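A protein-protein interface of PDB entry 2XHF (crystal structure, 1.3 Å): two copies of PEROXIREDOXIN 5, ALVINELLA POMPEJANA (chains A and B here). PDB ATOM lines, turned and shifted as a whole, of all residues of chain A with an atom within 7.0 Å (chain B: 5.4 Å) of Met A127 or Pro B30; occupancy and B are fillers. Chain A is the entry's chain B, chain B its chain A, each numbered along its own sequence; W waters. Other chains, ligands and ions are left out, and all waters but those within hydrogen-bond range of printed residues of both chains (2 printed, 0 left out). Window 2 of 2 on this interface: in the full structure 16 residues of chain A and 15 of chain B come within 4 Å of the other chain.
The backbone NH of Gly A129 sits at hydrogen-bond distance from the side-chain sulfur of Met B110.
O of Met A127 sits close to SD of Met B110 (3.4 Å).
O of Leu A128 sits close to SD of Met B110 (3.6 Å).
No position is printed for both chains.
A ring nitrogen (NE2) of His B111 sits at hydrogen-bond distance from the side-chain hydroxyl of Tyr B26, at 3.1 Å.
The backbone carbonyl oxygen (O) of Asn A130 lies within hydrogen-bond range of the backbone NH (N) of Ser A125, 3.4 Å away.
The backbone carbonyl oxygen (O) of Leu A128 sits close to the side-chain amide oxygen (OD1) of Asn A130 (3.4 Å).
Among the printed residues, merely in contact across the chains: Met A127 with Pro B30 (3.1 Å), Ser A125 with His B111 (3.2 Å), Pro A56 with Phe B89 (3.3 Å), Lys A126 with His B111 (3.8 Å), Gly A129 with His B111 (3.8 Å), Lys A126 with Met B110 (3.8 Å) and Leu A128 with Phe B89 (3.9 Å).
Of the printed residues of chain B, Met A127 touches Pro B30 (3.1 Å) and Met B110 (3.3 Å).
Pro B30 touches just one residue of chain A: Met A127 (3.1 Å).
Of the printed residues of chain B, Lys A126 touches Met B110 (3.8 Å) and His B111 (3.8 Å).
Printed residues of chain B within 4 Å of Leu A128: Phe B89 (3.9 Å) and Met B110 (3.3 Å).
The nearest residue of chain B that does not touch Met A127 is Phe B89 (4.1 Å).
The nearest residue of chain A that does not touch Pro B30 is Leu A128 (4.2 Å).
Of the 11 printed residues of chain B, 4 touch a printed residue of chain A.
Printed residues of chain B that touch a printed residue of chain A: Pro B30, Phe B89, Met B110 and His B111.
Hydrophobic or aromatic side chains of chain A that line the printed part of chain B: Pro A56, Met A127 and Leu A128.
Water W2 lies within hydrogen-bond range of O of Lys A126 (2.5 Å), OH of Tyr B26 (2.6 Å) and NE2 of His B111 (3.2 Å).
Water W1 lies within hydrogen-bond range of O of Gly A129 (2.6 Å) and ND1 of His B111 (2.8 Å).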
ATOM      1  N   VAL A  51     -31.188  -4.081 -16.101  1.00  0.00           N
ATOM      2  CA  VAL A  51     -30.275  -5.207 -15.902  1.00  0.00           C
ATOM      3  C   VAL A  51     -29.011  -4.738 -15.168  1.00  0.00           C
ATOM      4  O   VAL A  51     -28.442  -5.443 -14.325  1.00  0.00           O
ATOM      5  CB  VAL A  51     -29.942  -5.884 -17.232  1.00  0.00           C
ATOM      6  CG1 VAL A  51     -28.841  -6.938 -17.059  1.00  0.00           C
ATOM      7  CG2 VAL A  51     -31.208  -6.521 -17.806  1.00  0.00           C
ATOM      8  N   VAL A  55     -25.382  -0.970 -18.607  1.00  0.00           N
ATOM      9  CA  VAL A  55     -25.614  -2.114 -19.486  1.00  0.00           C
ATOM     10  C   VAL A  55     -26.429  -1.651 -20.689  1.00  0.00           C
ATOM     11  O   VAL A  55     -27.398  -0.932 -20.530  1.00  0.00           O
ATOM     12  CB  VAL A  55     -26.346  -3.236 -18.746  1.00  0.00           C
ATOM     13  CG1 VAL A  55     -26.723  -4.371 -19.692  1.00  0.00           C
ATOM     14  CG2 VAL A  55     -25.506  -3.735 -17.585  1.00  0.00           C
ATOM     15  N   PRO A  56     -26.024  -2.032 -21.917  1.00  0.00           N
ATOM     16  CA  PRO A  56     -26.814  -1.608 -23.076  1.00  0.00           C
ATOM     17  C   PRO A  56     -28.288  -1.978 -22.907  1.00  0.00           C
ATOM     18  O   PRO A  56     -28.617  -3.110 -22.555  1.00  0.00           O
ATOM     19  CB  PRO A  56     -26.157  -2.363 -24.243  1.00  0.00           C
ATOM     20  CG  PRO A  56     -24.754  -2.546 -23.819  1.00  0.00           C
ATOM     21  CD  PRO A  56     -24.807  -2.758 -22.335  1.00  0.00           C
ATOM     22  N   ASP A 123     -30.539 -15.326 -15.002  1.00  0.00           N
ATOM     23  CA  ASP A 123     -29.358 -16.200 -14.992  1.00  0.00           C
ATOM     24  C   ASP A 123     -28.257 -15.545 -15.826  1.00  0.00           C
ATOM     25  O   ASP A 123     -28.012 -15.933 -16.961  1.00  0.00           O
ATOM     26  CB  ASP A 123     -29.728 -17.581 -15.555  1.00  0.00           C
ATOM     27  CG  ASP A 123     -28.582 -18.574 -15.504  1.00  0.00           C
ATOM     28  OD1 ASP A 123     -27.531 -18.248 -14.920  1.00  0.00           O
ATOM     29  OD2 ASP A 123     -28.743 -19.695 -16.048  1.00  0.00           O
ATOM     30  N   SER A 124     -27.578 -14.563 -15.244  1.00  0.00           N
ATOM     31  CA  SER A 124     -26.675 -13.696 -15.987  1.00  0.00           C
ATOM     32  C   SER A 124     -25.238 -13.755 -15.484  1.00  0.00           C
ATOM     33  O   SER A 124     -24.428 -12.915 -15.848  1.00  0.00           O
ATOM     34  CB  SER A 124     -27.180 -12.252 -15.912  1.00  0.00           C
ATOM     35  OG  SER A 124     -27.300 -11.822 -14.570  1.00  0.00           O
ATOM     36  N   SER A 125     -24.923 -14.718 -14.624  1.00  0.00           N
ATOM     37  CA  SER A 125     -23.595 -14.757 -13.998  1.00  0.00           C
ATOM     38  C   SER A 125     -22.470 -14.873 -15.017  1.00  0.00           C
ATOM     39  O   SER A 125     -21.411 -14.307 -14.822  1.00  0.00           O
ATOM     40  CB  SER A 125     -23.478 -15.925 -13.019  1.00  0.00           C
ATOM     41  OG  SER A 125     -24.172 -15.635 -11.825  1.00  0.00           O
ATOM     42  N   LYS A 126     -22.684 -15.621 -16.093  1.00  0.00           N
ATOM     43  CA  LYS A 126     -21.620 -15.767 -17.080  1.00  0.00           C
ATOM     44  C   LYS A 126     -21.357 -14.471 -17.864  1.00  0.00           C
ATOM     45  O   LYS A 126     -20.219 -14.185 -18.240  1.00  0.00           O
ATOM     46  CB  LYS A 126     -21.943 -16.923 -18.026  1.00  0.00           C
ATOM     47  CG  LYS A 126     -20.705 -17.649 -18.520  1.00  0.00           C
ATOM     48  CD  LYS A 126     -19.869 -18.179 -17.349  1.00  0.00           C
ATOM     49  CE  LYS A 126     -18.393 -18.293 -17.703  1.00  0.00           C
ATOM     50  NZ  LYS A 126     -17.532 -18.211 -16.490  1.00  0.00           N
ATOM     51  N   MET A 127     -22.405 -13.696 -18.118  1.00  0.00           N
ATOM     52  CA  MET A 127     -22.309 -12.449 -18.875  1.00  0.00           C
ATOM     53  C   MET A 127     -21.862 -11.270 -17.990  1.00  0.00           C
ATOM     54  O   MET A 127     -21.153 -10.382 -18.453  1.00  0.00           O
ATOM     55  CB  MET A 127     -23.688 -12.120 -19.506  1.00  0.00           C
ATOM     56  CG  MET A 127     -23.776 -10.788 -20.304  1.00  0.00           C
ATOM     57  SD  MET A 127     -25.445 -10.323 -20.898  1.00  0.00           S
ATOM     58  CE  MET A 127     -25.124  -8.718 -21.627  1.00  0.00           C
ATOM     59  N   LEU A 128     -22.292 -11.250 -16.722  1.00  0.00           N
ATOM     60  CA  LEU A 128     -22.124 -10.062 -15.906  1.00  0.00           C
ATOM     61  C   LEU A 128     -21.563 -10.310 -14.522  1.00  0.00           C
ATOM     62  O   LEU A 128     -21.490  -9.377 -13.721  1.00  0.00           O
ATOM     63  CB  LEU A 128     -23.465  -9.349 -15.771  1.00  0.00           C
ATOM     64  CG  LEU A 128     -24.031  -8.754 -17.062  1.00  0.00           C
ATOM     65  CD1 LEU A 128     -25.453  -8.237 -16.828  1.00  0.00           C
ATOM     66  CD2 LEU A 128     -23.148  -7.636 -17.598  1.00  0.00           C
ATOM     67  N   GLY A 129     -21.174 -11.544 -14.238  1.00  0.00           N
ATOM     68  CA  GLY A 129     -20.512 -11.875 -12.991  1.00  0.00           C
ATOM     69  C   GLY A 129     -21.398 -12.336 -11.856  1.00  0.00           C
ATOM     70  O   GLY A 129     -20.960 -13.077 -10.967  1.00  0.00           O
ATOM     71  N   ASN A 130     -22.642 -11.885 -11.898  1.00  0.00           N
ATOM     72  CA  ASN A 130     -23.662 -12.235 -10.911  1.00  0.00           C
ATOM     73  C   ASN A 130     -25.045 -12.217 -11.546  1.00  0.00           C
ATOM     74  O   ASN A 130     -25.198 -11.876 -12.716  1.00  0.00           O
ATOM     75  CB  ASN A 130     -23.618 -11.291  -9.686  1.00  0.00           C
ATOM     76  CG  ASN A 130     -23.856  -9.821 -10.040  1.00  0.00           C
ATOM     77  OD1 ASN A 130     -23.738  -9.409 -11.187  1.00  0.00           O
ATOM     78  ND2 ASN A 130     -24.185  -9.025  -9.032  1.00  0.00           N
ATOM     79  N   TYR B  26     -11.976  -9.271 -18.857  1.00  0.00           N
ATOM     80  CA  TYR B  26     -12.924  -8.706 -19.801  1.00  0.00           C
ATOM     81  C   TYR B  26     -12.595  -7.245 -20.034  1.00  0.00           C
ATOM     82  O   TYR B  26     -12.024  -6.581 -19.163  1.00  0.00           O
ATOM     83  CB  TYR B  26     -14.347  -8.853 -19.241  1.00  0.00           C
ATOM     84  CG  TYR B  26     -14.714 -10.274 -18.992  1.00  0.00           C
ATOM     85  CD1 TYR B  26     -14.244 -10.950 -17.864  1.00  0.00           C
ATOM     86  CD2 TYR B  26     -15.528 -10.964 -19.879  1.00  0.00           C
ATOM     87  CE1 TYR B  26     -14.560 -12.277 -17.655  1.00  0.00           C
ATOM     88  CE2 TYR B  26     -15.842 -12.278 -19.678  1.00  0.00           C
ATOM     89  CZ  TYR B  26     -15.368 -12.933 -18.564  1.00  0.00           C
ATOM     90  OH  TYR B  26     -15.701 -14.253 -18.367  1.00  0.00           O
ATOM     91  N   ASP B  28     -14.387  -3.739 -22.055  1.00  0.00           N
ATOM     92  CA  ASP B  28     -15.471  -3.089 -22.818  1.00  0.00           C
ATOM     93  C   ASP B  28     -16.837  -3.801 -22.773  1.00  0.00           C
ATOM     94  O   ASP B  28     -17.836  -3.219 -22.334  1.00  0.00           O
ATOM     95  CB  ASP B  28     -15.068  -2.826 -24.265  1.00  0.00           C
ATOM     96  CG  ASP B  28     -13.887  -1.887 -24.376  1.00  0.00           C
ATOM     97  OD1 ASP B  28     -13.978  -0.768 -23.841  1.00  0.00           O
ATOM     98  OD2 ASP B  28     -12.865  -2.260 -24.995  1.00  0.00           O
ATOM     99  N   VAL B  29     -16.876  -5.055 -23.200  1.00  0.00           N
ATOM    100  CA  VAL B  29     -18.121  -5.811 -23.254  1.00  0.00           C
ATOM    101  C   VAL B  29     -17.859  -7.253 -22.847  1.00  0.00           C
ATOM    102  O   VAL B  29     -16.741  -7.733 -22.982  1.00  0.00           O
ATOM    103  CB  VAL B  29     -18.749  -5.777 -24.668  1.00  0.00           C
ATOM    104  CG1 VAL B  29     -19.135  -4.341 -25.054  1.00  0.00           C
ATOM    105  CG2 VAL B  29     -17.791  -6.378 -25.696  1.00  0.00           C
ATOM    106  N   PRO B  30     -18.885  -7.954 -22.344  1.00  0.00           N
ATOM    107  CA  PRO B  30     -18.662  -9.314 -21.839  1.00  0.00           C
ATOM    108  C   PRO B  30     -18.188 -10.302 -22.900  1.00  0.00           C
ATOM    109  O   PRO B  30     -17.523 -11.289 -22.561  1.00  0.00           O
ATOM    110  CB  PRO B  30     -20.027  -9.713 -21.263  1.00  0.00           C
ATOM    111  CG  PRO B  30     -20.687  -8.405 -20.934  1.00  0.00           C
ATOM    112  CD  PRO B  30     -20.231  -7.456 -22.010  1.00  0.00           C
ATOM    113  N   SER B  31     -18.514 -10.039 -24.163  1.00  0.00           N
ATOM    114  CA  SER B  31     -18.072 -10.917 -25.249  1.00  0.00           C
ATOM    115  C   SER B  31     -16.571 -10.749 -25.578  1.00  0.00           C
ATOM    116  O   SER B  31     -15.970 -11.598 -26.252  1.00  0.00           O
ATOM    117  CB  SER B  31     -18.953 -10.705 -26.493  1.00  0.00           C
ATOM    118  OG  SER B  31     -18.764  -9.428 -27.070  1.00  0.00           O
ATOM    119  N   LYS B  32     -15.964  -9.661 -25.095  1.00  0.00           N
ATOM    120  CA  LYS B  32     -14.536  -9.427 -25.320  1.00  0.00           C
ATOM    121  C   LYS B  32     -13.751  -9.846 -24.099  1.00  0.00           C
ATOM    122  O   LYS B  32     -13.591  -9.074 -23.151  1.00  0.00           O
ATOM    123  CB  LYS B  32     -14.235  -7.971 -25.664  1.00  0.00           C
ATOM    124  CG  LYS B  32     -12.731  -7.687 -25.825  1.00  0.00           C
ATOM    125  CD  LYS B  32     -12.387  -6.206 -25.851  1.00  0.00           C
ATOM    126  CE  LYS B  32     -13.024  -5.480 -27.005  1.00  0.00           C
ATOM    127  NZ  LYS B  32     -12.623  -4.047 -26.967  1.00  0.00           N
ATOM    128  N   SER B  33     -13.319 -11.099 -24.102  1.00  0.00           N
ATOM    129  CA  SER B  33     -12.489 -11.605 -23.025  1.00  0.00           C
ATOM    130  C   SER B  33     -11.247 -12.278 -23.587  1.00  0.00           C
ATOM    131  O   SER B  33     -11.212 -12.743 -24.726  1.00  0.00           O
ATOM    132  CB  SER B  33     -13.242 -12.578 -22.146  1.00  0.00           C
ATOM    133  OG  SER B  33     -13.707 -13.654 -22.915  1.00  0.00           O
ATOM    134  N   PRO B  88     -17.617  -5.382 -17.337  1.00  0.00           N
ATOM    135  CA  PRO B  88     -16.893  -4.505 -18.258  1.00  0.00           C
ATOM    136  C   PRO B  88     -17.666  -3.300 -18.756  1.00  0.00           C
ATOM    137  O   PRO B  88     -17.044  -2.326 -19.126  1.00  0.00           O
ATOM    138  CB  PRO B  88     -16.531  -5.436 -19.418  1.00  0.00           C
ATOM    139  CG  PRO B  88     -17.531  -6.534 -19.334  1.00  0.00           C
ATOM    140  CD  PRO B  88     -17.797  -6.736 -17.878  1.00  0.00           C
ATOM    141  N   PHE B  89     -18.997  -3.325 -18.732  1.00  0.00           N
ATOM    142  CA  PHE B  89     -19.747  -2.121 -19.134  1.00  0.00           C
ATOM    143  C   PHE B  89     -19.472  -0.996 -18.137  1.00  0.00           C
ATOM    144  O   PHE B  89     -19.167   0.150 -18.507  1.00  0.00           O
ATOM    145  CB  PHE B  89     -21.240  -2.388 -19.208  1.00  0.00           C
ATOM    146  CG  PHE B  89     -21.644  -3.399 -20.247  1.00  0.00           C
ATOM    147  CD1 PHE B  89     -21.384  -3.181 -21.596  1.00  0.00           C
ATOM    148  CD2 PHE B  89     -22.314  -4.559 -19.881  1.00  0.00           C
ATOM    149  CE1 PHE B  89     -21.834  -4.085 -22.554  1.00  0.00           C
ATOM    150  CE2 PHE B  89     -22.776  -5.456 -20.839  1.00  0.00           C
ATOM    151  CZ  PHE B  89     -22.494  -5.220 -22.173  1.00  0.00           C
ATOM    152  N   MET B 110     -14.228  -9.724 -13.779  1.00  0.00           N
ATOM    153  CA  MET B 110     -15.652  -9.680 -13.481  1.00  0.00           C
ATOM    154  C   MET B 110     -16.102 -10.720 -12.463  1.00  0.00           C
ATOM    155  O   MET B 110     -17.011 -10.458 -11.673  1.00  0.00           O
ATOM    156  CB  MET B 110     -16.441  -9.842 -14.781  1.00  0.00           C
ATOM    157  CG  MET B 110     -17.927  -9.856 -14.574  1.00  0.00           C
ATOM    158  SD  MET B 110     -18.786  -9.738 -16.132  1.00  0.00           S
ATOM    159  CE  MET B 110     -18.259 -11.160 -16.966  1.00  0.00           C
ATOM    160  N   HIS B 111     -15.504 -11.905 -12.515  1.00  0.00           N
ATOM    161  CA  HIS B 111     -15.855 -12.983 -11.596  1.00  0.00           C
ATOM    162  C   HIS B 111     -14.958 -12.981 -10.365  1.00  0.00           C
ATOM    163  O   HIS B 111     -15.097 -13.842  -9.498  1.00  0.00           O
ATOM    164  CB  HIS B 111     -15.710 -14.344 -12.296  1.00  0.00           C
ATOM    165  CG  HIS B 111     -16.478 -14.451 -13.571  1.00  0.00           C
ATOM    166  ND1 HIS B 111     -17.855 -14.512 -13.613  1.00  0.00           N
ATOM    167  CD2 HIS B 111     -16.060 -14.459 -14.855  1.00  0.00           C
ATOM    168  CE1 HIS B 111     -18.251 -14.594 -14.869  1.00  0.00           C
ATOM    169  NE2 HIS B 111     -17.181 -14.558 -15.644  1.00  0.00           N
HETATM  170  O   HOH W   1     -19.230 -15.012 -11.218  1.00  0.00           O
HETATM  171  O   HOH W   2     -18.048 -15.376 -18.663  1.00  0.00           O
